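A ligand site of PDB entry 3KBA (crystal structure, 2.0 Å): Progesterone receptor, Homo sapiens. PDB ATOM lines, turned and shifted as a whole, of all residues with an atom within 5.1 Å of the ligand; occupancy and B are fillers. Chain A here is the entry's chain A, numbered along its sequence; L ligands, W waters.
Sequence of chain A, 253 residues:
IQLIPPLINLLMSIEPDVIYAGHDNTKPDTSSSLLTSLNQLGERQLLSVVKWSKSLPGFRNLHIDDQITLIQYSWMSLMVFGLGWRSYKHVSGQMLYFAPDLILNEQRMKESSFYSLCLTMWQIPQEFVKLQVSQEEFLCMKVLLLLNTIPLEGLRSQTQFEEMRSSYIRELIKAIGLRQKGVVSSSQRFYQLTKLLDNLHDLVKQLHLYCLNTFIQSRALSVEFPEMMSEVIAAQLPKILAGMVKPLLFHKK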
ATOM      1  N   LEU A  35      10.655 -28.830 -32.201  1.00  0.00           N
ATOM      2  CA  LEU A  35      10.627 -27.437 -31.735  1.00  0.00           C
ATOM      3  C   LEU A  35      10.773 -26.444 -32.894  1.00  0.00           C
ATOM      4  O   LEU A  35      10.114 -25.409 -32.908  1.00  0.00           O
ATOM      5  CB  LEU A  35      11.709 -27.172 -30.667  1.00  0.00           C
ATOM      6  CG  LEU A  35      11.417 -27.700 -29.261  1.00  0.00           C
ATOM      7  CD1 LEU A  35      12.588 -27.445 -28.337  1.00  0.00           C
ATOM      8  CD2 LEU A  35      10.146 -27.078 -28.691  1.00  0.00           C
ATOM      9  N   LEU A  38       7.432 -26.383 -34.664  1.00  0.00           N
ATOM     10  CA  LEU A  38       6.515 -25.584 -33.851  1.00  0.00           C
ATOM     11  C   LEU A  38       6.831 -24.084 -33.949  1.00  0.00           C
ATOM     12  O   LEU A  38       5.917 -23.262 -33.945  1.00  0.00           O
ATOM     13  CB  LEU A  38       6.559 -26.044 -32.388  1.00  0.00           C
ATOM     14  CG  LEU A  38       5.935 -27.426 -32.139  1.00  0.00           C
ATOM     15  CD1 LEU A  38       6.322 -27.989 -30.772  1.00  0.00           C
ATOM     16  CD2 LEU A  38       4.412 -27.361 -32.282  1.00  0.00           C
ATOM     17  N   ASN A  39       8.108 -23.734 -34.064  1.00  0.00           N
ATOM     18  CA  ASN A  39       8.498 -22.344 -34.287  1.00  0.00           C
ATOM     19  C   ASN A  39       8.074 -21.851 -35.675  1.00  0.00           C
ATOM     20  O   ASN A  39       7.692 -20.684 -35.834  1.00  0.00           O
ATOM     21  CB  ASN A  39      10.016 -22.171 -34.107  1.00  0.00           C
ATOM     22  CG  ASN A  39      10.433 -22.230 -32.644  1.00  0.00           C
ATOM     23  OD1 ASN A  39       9.613 -22.058 -31.750  1.00  0.00           O
ATOM     24  ND2 ASN A  39      11.713 -22.470 -32.415  1.00  0.00           N
ATOM     25  N   LEU A  41       5.461 -23.065 -37.316  1.00  0.00           N
ATOM     26  CA  LEU A  41       4.022 -22.885 -37.123  1.00  0.00           C
ATOM     27  C   LEU A  41       3.721 -21.564 -36.400  1.00  0.00           C
ATOM     28  O   LEU A  41       2.779 -20.865 -36.742  1.00  0.00           O
ATOM     29  CB  LEU A  41       3.432 -24.067 -36.350  1.00  0.00           C
ATOM     30  CG  LEU A  41       1.924 -24.033 -36.045  1.00  0.00           C
ATOM     31  CD1 LEU A  41       1.105 -23.996 -37.332  1.00  0.00           C
ATOM     32  CD2 LEU A  41       1.545 -25.237 -35.186  1.00  0.00           C
ATOM     33  N   GLY A  42       4.538 -21.239 -35.389  1.00  0.00           N
ATOM     34  CA  GLY A  42       4.370 -20.007 -34.618  1.00  0.00           C
ATOM     35  C   GLY A  42       4.536 -18.743 -35.439  1.00  0.00           C
ATOM     36  O   GLY A  42       3.848 -17.755 -35.212  1.00  0.00           O
ATOM     37  N   GLN A  45       1.318 -18.621 -37.547  1.00  0.00           N
ATOM     38  CA  GLN A  45       0.224 -18.236 -36.659  1.00  0.00           C
ATOM     39  C   GLN A  45       0.261 -16.739 -36.332  1.00  0.00           C
ATOM     40  O   GLN A  45      -0.777 -16.077 -36.316  1.00  0.00           O
ATOM     41  CB  GLN A  45       0.280 -19.044 -35.360  1.00  0.00           C
ATOM     42  CG  GLN A  45      -0.161 -20.497 -35.516  1.00  0.00           C
ATOM     43  CD  GLN A  45      -1.671 -20.664 -35.485  1.00  0.00           C
ATOM     44  OE1 GLN A  45      -2.394 -19.876 -34.848  1.00  0.00           O
ATOM     45  NE2 GLN A  45      -2.173 -21.703 -36.148  1.00  0.00           N
ATOM     46  N   TRP A  75       0.202 -13.070 -28.169  1.00  0.00           N
ATOM     47  CA  TRP A  75       0.666 -14.020 -29.183  1.00  0.00           C
ATOM     48  C   TRP A  75       0.588 -15.484 -28.700  1.00  0.00           C
ATOM     49  O   TRP A  75      -0.069 -16.314 -29.331  1.00  0.00           O
ATOM     50  CB  TRP A  75       2.094 -13.667 -29.625  1.00  0.00           C
ATOM     51  CG  TRP A  75       2.783 -14.745 -30.394  1.00  0.00           C
ATOM     52  CD1 TRP A  75       2.428 -15.234 -31.614  1.00  0.00           C
ATOM     53  CD2 TRP A  75       3.945 -15.468 -29.998  1.00  0.00           C
ATOM     54  NE1 TRP A  75       3.297 -16.219 -32.007  1.00  0.00           N
ATOM     55  CE2 TRP A  75       4.245 -16.385 -31.023  1.00  0.00           C
ATOM     56  CE3 TRP A  75       4.773 -15.429 -28.866  1.00  0.00           C
ATOM     57  CZ2 TRP A  75       5.344 -17.253 -30.961  1.00  0.00           C
ATOM     58  CZ3 TRP A  75       5.861 -16.288 -28.801  1.00  0.00           C
ATOM     59  CH2 TRP A  75       6.126 -17.197 -29.847  1.00  0.00           C
ATOM     60  N   MET A  76       1.251 -15.783 -27.599  1.00  0.00           N
ATOM     61  CA  MET A  76       1.243 -17.132 -27.034  1.00  0.00           C
ATOM     62  C   MET A  76      -0.154 -17.591 -26.602  1.00  0.00           C
ATOM     63  O   MET A  76      -0.562 -18.710 -26.903  1.00  0.00           O
ATOM     64  CB  MET A  76       2.215 -17.228 -25.848  1.00  0.00           C
ATOM     65  CG  MET A  76       2.421 -18.633 -25.300  1.00  0.00           C
ATOM     66  SD  MET A  76       3.287 -19.730 -26.447  1.00  0.00           S
ATOM     67  CE  MET A  76       4.974 -19.146 -26.243  1.00  0.00           C
ATOM     68  N   MET A  79      -2.348 -18.519 -29.560  1.00  0.00           N
ATOM     69  CA  MET A  79      -1.900 -19.773 -30.155  1.00  0.00           C
ATOM     70  C   MET A  79      -2.404 -20.979 -29.369  1.00  0.00           C
ATOM     71  O   MET A  79      -2.992 -21.887 -29.949  1.00  0.00           O
ATOM     72  CB  MET A  79      -0.365 -19.831 -30.259  1.00  0.00           C
ATOM     73  CG  MET A  79       0.199 -19.005 -31.406  1.00  0.00           C
ATOM     74  SD  MET A  79       1.856 -19.523 -31.886  1.00  0.00           S
ATOM     75  CE  MET A  79       2.742 -19.479 -30.335  1.00  0.00           C
ATOM     76  N   VAL A  80      -2.190 -20.966 -28.058  1.00  0.00           N
ATOM     77  CA  VAL A  80      -2.606 -22.071 -27.187  1.00  0.00           C
ATOM     78  C   VAL A  80      -4.121 -22.199 -27.083  1.00  0.00           C
ATOM     79  O   VAL A  80      -4.644 -23.301 -26.943  1.00  0.00           O
ATOM     80  CB  VAL A  80      -1.967 -21.950 -25.760  1.00  0.00           C
ATOM     81  CG1 VAL A  80      -2.628 -20.835 -24.965  1.00  0.00           C
ATOM     82  CG2 VAL A  80      -2.067 -23.261 -25.008  1.00  0.00           C
ATOM     83  N   LEU A  83      -5.037 -23.817 -30.342  1.00  0.00           N
ATOM     84  CA  LEU A  83      -4.673 -25.210 -30.161  1.00  0.00           C
ATOM     85  C   LEU A  83      -5.760 -25.965 -29.394  1.00  0.00           C
ATOM     86  O   LEU A  83      -6.102 -27.107 -29.728  1.00  0.00           O
ATOM     87  CB  LEU A  83      -3.335 -25.326 -29.425  1.00  0.00           C
ATOM     88  CG  LEU A  83      -2.922 -26.710 -28.919  1.00  0.00           C
ATOM     89  CD1 LEU A  83      -2.680 -27.677 -30.086  1.00  0.00           C
ATOM     90  CD2 LEU A  83      -1.689 -26.593 -28.034  1.00  0.00           C
ATOM     91  N   ARG A  86      -8.827 -26.539 -31.891  1.00  0.00           N
ATOM     92  CA  ARG A  86      -8.563 -27.544 -32.914  1.00  0.00           C
ATOM     93  C   ARG A  86      -8.469 -28.955 -32.332  1.00  0.00           C
ATOM     94  O   ARG A  86      -8.977 -29.901 -32.919  1.00  0.00           O
ATOM     95  CB  ARG A  86      -7.289 -27.199 -33.687  1.00  0.00           C
ATOM     96  CG  ARG A  86      -7.408 -25.964 -34.567  1.00  0.00           C
ATOM     97  CD  ARG A  86      -6.220 -25.814 -35.515  1.00  0.00           C
ATOM     98  NE  ARG A  86      -4.959 -25.700 -34.778  1.00  0.00           N
ATOM     99  CZ  ARG A  86      -4.547 -24.601 -34.152  1.00  0.00           C
ATOM    100  NH1 ARG A  86      -5.282 -23.491 -34.156  1.00  0.00           N
ATOM    101  NH2 ARG A  86      -3.384 -24.597 -33.511  1.00  0.00           N
ATOM    102  N   PHE A  98      -1.839 -29.242 -33.243  1.00  0.00           N
ATOM    103  CA  PHE A  98      -1.149 -27.979 -33.541  1.00  0.00           C
ATOM    104  C   PHE A  98      -1.450 -27.559 -34.983  1.00  0.00           C
ATOM    105  O   PHE A  98      -1.733 -26.388 -35.254  1.00  0.00           O
ATOM    106  CB  PHE A  98       0.360 -28.114 -33.322  1.00  0.00           C
ATOM    107  CG  PHE A  98       0.756 -28.226 -31.871  1.00  0.00           C
ATOM    108  CD1 PHE A  98       0.936 -29.465 -31.275  1.00  0.00           C
ATOM    109  CD2 PHE A  98       0.959 -27.079 -31.110  1.00  0.00           C
ATOM    110  CE1 PHE A  98       1.314 -29.557 -29.932  1.00  0.00           C
ATOM    111  CE2 PHE A  98       1.337 -27.171 -29.767  1.00  0.00           C
ATOM    112  CZ  PHE A  98       1.507 -28.419 -29.182  1.00  0.00           C
ATOM    113  N   PHE A 114       9.320 -30.331 -21.740  1.00  0.00           N
ATOM    114  CA  PHE A 114       8.528 -30.203 -22.960  1.00  0.00           C
ATOM    115  C   PHE A 114       7.210 -30.971 -22.863  1.00  0.00           C
ATOM    116  O   PHE A 114       6.148 -30.425 -23.158  1.00  0.00           O
ATOM    117  CB  PHE A 114       9.327 -30.683 -24.183  1.00  0.00           C
ATOM    118  CG  PHE A 114       8.601 -30.476 -25.488  1.00  0.00           C
ATOM    119  CD1 PHE A 114       8.449 -29.201 -26.021  1.00  0.00           C
ATOM    120  CD2 PHE A 114       8.067 -31.565 -26.183  1.00  0.00           C
ATOM    121  CE1 PHE A 114       7.788 -29.014 -27.226  1.00  0.00           C
ATOM    122  CE2 PHE A 114       7.395 -31.369 -27.385  1.00  0.00           C
ATOM    123  CZ  PHE A 114       7.257 -30.102 -27.907  1.00  0.00           C
ATOM    124  N   LEU A 117       5.055 -29.190 -20.271  1.00  0.00           N
ATOM    125  CA  LEU A 117       4.338 -28.038 -20.817  1.00  0.00           C
ATOM    126  C   LEU A 117       3.197 -28.470 -21.730  1.00  0.00           C
ATOM    127  O   LEU A 117       2.131 -27.858 -21.732  1.00  0.00           O
ATOM    128  CB  LEU A 117       5.282 -27.089 -21.577  1.00  0.00           C
ATOM    129  CG  LEU A 117       6.129 -26.102 -20.755  1.00  0.00           C
ATOM    130  CD1 LEU A 117       5.272 -25.263 -19.830  1.00  0.00           C
ATOM    131  CD2 LEU A 117       7.215 -26.820 -19.982  1.00  0.00           C
ATOM    132  N   CYS A 118       3.413 -29.534 -22.512  1.00  0.00           N
ATOM    133  CA  CYS A 118       2.355 -30.088 -23.353  1.00  0.00           C
ATOM    134  C   CYS A 118       1.160 -30.538 -22.508  1.00  0.00           C
ATOM    135  O   CYS A 118       0.010 -30.332 -22.900  1.00  0.00           O
ATOM    136  CB  CYS A 118       2.874 -31.240 -24.206  1.00  0.00           C
ATOM    137  SG  CYS A 118       3.894 -30.700 -25.589  1.00  0.00           S
ATOM    138  N   MET A 121      -0.696 -27.310 -21.419  1.00  0.00           N
ATOM    139  CA  MET A 121      -1.443 -26.836 -22.589  1.00  0.00           C
ATOM    140  C   MET A 121      -2.674 -27.702 -22.845  1.00  0.00           C
ATOM    141  O   MET A 121      -3.713 -27.196 -23.255  1.00  0.00           O
ATOM    142  CB  MET A 121      -0.559 -26.855 -23.840  1.00  0.00           C
ATOM    143  CG  MET A 121       0.452 -25.740 -23.929  1.00  0.00           C
ATOM    144  SD  MET A 121       1.272 -25.713 -25.533  1.00  0.00           S
ATOM    145  CE  MET A 121       2.278 -27.176 -25.386  1.00  0.00           C
ATOM    146  N   LEU A 207       4.511 -21.073 -20.259  1.00  0.00           N
ATOM    147  CA  LEU A 207       4.815 -21.176 -21.691  1.00  0.00           C
ATOM    148  C   LEU A 207       5.750 -20.066 -22.156  1.00  0.00           C
ATOM    149  O   LEU A 207       6.662 -20.304 -22.947  1.00  0.00           O
ATOM    150  CB  LEU A 207       3.523 -21.160 -22.508  1.00  0.00           C
ATOM    151  CG  LEU A 207       2.509 -22.290 -22.262  1.00  0.00           C
ATOM    152  CD1 LEU A 207       1.283 -22.082 -23.135  1.00  0.00           C
ATOM    153  CD2 LEU A 207       3.132 -23.655 -22.517  1.00  0.00           C
ATOM    154  N   TYR A 210       9.401 -20.948 -20.695  1.00  0.00           N
ATOM    155  CA  TYR A 210      10.011 -22.011 -21.493  1.00  0.00           C
ATOM    156  C   TYR A 210      10.466 -21.482 -22.860  1.00  0.00           C
ATOM    157  O   TYR A 210      11.555 -21.825 -23.328  1.00  0.00           O
ATOM    158  CB  TYR A 210       9.022 -23.164 -21.682  1.00  0.00           C
ATOM    159  CG  TYR A 210       9.625 -24.344 -22.410  1.00  0.00           C
ATOM    160  CD1 TYR A 210       9.069 -24.811 -23.601  1.00  0.00           C
ATOM    161  CD2 TYR A 210      10.743 -24.990 -21.918  1.00  0.00           C
ATOM    162  CE1 TYR A 210       9.621 -25.909 -24.276  1.00  0.00           C
ATOM    163  CE2 TYR A 210      11.305 -26.080 -22.581  1.00  0.00           C
ATOM    164  CZ  TYR A 210      10.732 -26.528 -23.754  1.00  0.00           C
ATOM    165  OH  TYR A 210      11.305 -27.608 -24.406  1.00  0.00           O
ATOM    166  N   CYS A 211       9.636 -20.654 -23.474  1.00  0.00           N
ATOM    167  CA  CYS A 211       9.966 -20.057 -24.771  1.00  0.00           C
ATOM    168  C   CYS A 211      11.215 -19.172 -24.708  1.00  0.00           C
ATOM    169  O   CYS A 211      12.121 -19.322 -25.519  1.00  0.00           O
ATOM    170  CB  CYS A 211       8.775 -19.257 -25.290  1.00  0.00           C
ATOM    171  SG  CYS A 211       9.071 -18.380 -26.826  1.00  0.00           S
ATOM    172  N   THR A 214      14.353 -21.231 -24.127  1.00  0.00           N
ATOM    173  CA  THR A 214      14.721 -21.948 -25.350  1.00  0.00           C
ATOM    174  C   THR A 214      15.309 -20.992 -26.395  1.00  0.00           C
ATOM    175  O   THR A 214      16.219 -21.357 -27.133  1.00  0.00           O
ATOM    176  CB  THR A 214      13.511 -22.685 -25.939  1.00  0.00           C
ATOM    177  OG1 THR A 214      12.897 -23.487 -24.927  1.00  0.00           O
ATOM    178  CG2 THR A 214      13.935 -23.573 -27.108  1.00  0.00           C
ATOM    179  N   VAL A 223      17.816 -25.180 -32.388  1.00  0.00           N
ATOM    180  CA  VAL A 223      16.411 -24.848 -32.676  1.00  0.00           C
ATOM    181  C   VAL A 223      16.350 -23.485 -33.375  1.00  0.00           C
ATOM    182  O   VAL A 223      16.825 -22.488 -32.834  1.00  0.00           O
ATOM    183  CB  VAL A 223      15.578 -24.803 -31.383  1.00  0.00           C
ATOM    184  CG1 VAL A 223      14.161 -24.325 -31.654  1.00  0.00           C
ATOM    185  CG2 VAL A 223      15.565 -26.179 -30.704  1.00  0.00           C
ATOM    186  N   PHE A 225      14.541 -20.145 -34.730  1.00  0.00           N
ATOM    187  CA  PHE A 225      13.443 -19.233 -34.396  1.00  0.00           C
ATOM    188  C   PHE A 225      13.301 -18.235 -35.549  1.00  0.00           C
ATOM    189  O   PHE A 225      14.175 -17.384 -35.740  1.00  0.00           O
ATOM    190  CB  PHE A 225      13.738 -18.468 -33.110  1.00  0.00           C
ATOM    191  CG  PHE A 225      13.523 -19.260 -31.856  1.00  0.00           C
ATOM    192  CD1 PHE A 225      14.464 -20.193 -31.431  1.00  0.00           C
ATOM    193  CD2 PHE A 225      12.383 -19.071 -31.088  1.00  0.00           C
ATOM    194  CE1 PHE A 225      14.269 -20.924 -30.269  1.00  0.00           C
ATOM    195  CE2 PHE A 225      12.178 -19.793 -29.923  1.00  0.00           C
ATOM    196  CZ  PHE A 225      13.120 -20.720 -29.514  1.00  0.00           C
ATOM    197  N   MET A 229       8.401 -13.910 -35.039  1.00  0.00           N
ATOM    198  CA  MET A 229       8.172 -14.384 -33.678  1.00  0.00           C
ATOM    199  C   MET A 229       9.389 -14.153 -32.759  1.00  0.00           C
ATOM    200  O   MET A 229       9.216 -13.975 -31.557  1.00  0.00           O
ATOM    201  CB  MET A 229       7.694 -15.849 -33.667  1.00  0.00           C
ATOM    202  CG  MET A 229       8.604 -16.856 -34.366  1.00  0.00           C
ATOM    203  SD  MET A 229       9.804 -17.630 -33.275  1.00  0.00           S
ATOM    204  CE  MET A 229       8.708 -18.553 -32.183  1.00  0.00           C
HETATM  205  C1  LIG L   1       5.896 -23.157 -25.076  1.00  0.00           C
HETATM  206  C2  LIG L   1       5.602 -24.395 -25.855  1.00  0.00           C
HETATM  207  C3  LIG L   1       5.637 -25.621 -25.202  1.00  0.00           C
HETATM  208  C4  LIG L   1       5.336 -26.790 -25.902  1.00  0.00           C
HETATM  209  C5  LIG L   1       5.054 -26.737 -27.256  1.00  0.00           C
HETATM  210  C6  LIG L   1       5.003 -25.510 -27.905  1.00  0.00           C
HETATM  211  C7  LIG L   1       5.306 -24.335 -27.221  1.00  0.00           C
HETATM  212  C8  LIG L   1       5.238 -23.040 -27.943  1.00  0.00           C
HETATM  213  N1  LIG L   1       5.200 -23.045 -29.375  1.00  0.00           N
HETATM  214  C9  LIG L   1       6.357 -22.661 -30.108  1.00  0.00           C
HETATM  215  C10 LIG L   1       6.863 -21.268 -29.900  1.00  0.00           C
HETATM  216  C11 LIG L   1       8.072 -21.434 -28.973  1.00  0.00           C
HETATM  217  N2  LIG L   1       8.376 -22.848 -28.928  1.00  0.00           N
HETATM  218  C12 LIG L   1       7.540 -23.531 -29.923  1.00  0.00           C
HETATM  219  S1  LIG L   1       9.751 -22.937 -28.094  1.00  0.00           S
HETATM  220  C13 LIG L   1       9.564 -24.040 -26.760  1.00  0.00           C
HETATM  221  O1  LIG L   1      10.098 -21.633 -27.647  1.00  0.00           O
HETATM  222  O2  LIG L   1      10.768 -23.434 -28.944  1.00  0.00           O
HETATM  223  C14 LIG L   1       3.958 -23.143 -30.052  1.00  0.00           C
HETATM  224  C15 LIG L   1       3.921 -23.100 -31.451  1.00  0.00           C
HETATM  225  C16 LIG L   1       2.708 -23.166 -32.123  1.00  0.00           C
HETATM  226  C17 LIG L   1       1.531 -23.292 -31.410  1.00  0.00           C
HETATM  227  C18 LIG L   1       0.235 -23.356 -32.154  1.00  0.00           C
HETATM  228  N3  LIG L   1      -0.742 -23.418 -32.720  1.00  0.00           N
HETATM  229  C19 LIG L   1       1.563 -23.372 -30.015  1.00  0.00           C
HETATM  230 CL1  LIG L   1       0.118 -23.418 -29.086  1.00  0.00          CL
HETATM  231  C20 LIG L   1       2.770 -23.260 -29.336  1.00  0.00           C
HETATM  232  O   HOH W   1      -3.503 -21.468 -32.608  1.00  0.00           O
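The guanidinium group of Arg 86 lies within hydrogen-bond range of the backbone carbonyl oxygen of Phe 98 (3.0 Å). The backbone carbonyl oxygen of Tyr 210 sits at hydrogen-bond distance from the side-chain hydroxyl of Thr 214 (2.7 Å). ND2 of Asn 39 lies close to O of Leu 35, 3.4 Å away. The side-chain sulfur of Met 79 is in hydrogen-bond range of the indole nitrogen of Trp 75, 3.6 Å away. O of Phe 114 sits at hydrogen-bond distance from SG of Cys 118 (3.3 Å).
N3 of the ligand lies within hydrogen-bond range of NH2 of Arg 86, 3.0 Å away. The side-chain amide oxygen (OD1) of Asn 39 lies close to an oxygen (O2) of the ligand (3.3 Å). An oxygen (O1) of the ligand lies close to the side-chain sulfur (SG) of Cys 211.
Merely in contact with the ligand: Tyr 210, Met 121, Leu 38, Met 79, Val 80, Phe 114, Phe 225, Leu 207, Leu 35, Thr 214, Leu 41, Leu 83, Phe 98, Leu 117 and Met 229. 18 residues have an atom within 4 Å of the ligand: Leu 35, Leu 38, Asn 39, Leu 41, Met 79, Val 80, Leu 83, Arg 86, Phe 98, Phe 114, Leu 117, Met 121, Leu 207, Tyr 210, Cys 211, Thr 214, Phe 225 and Met 229. Along chain A the residues within 4 Å of the ligand span positions 35 to 229.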
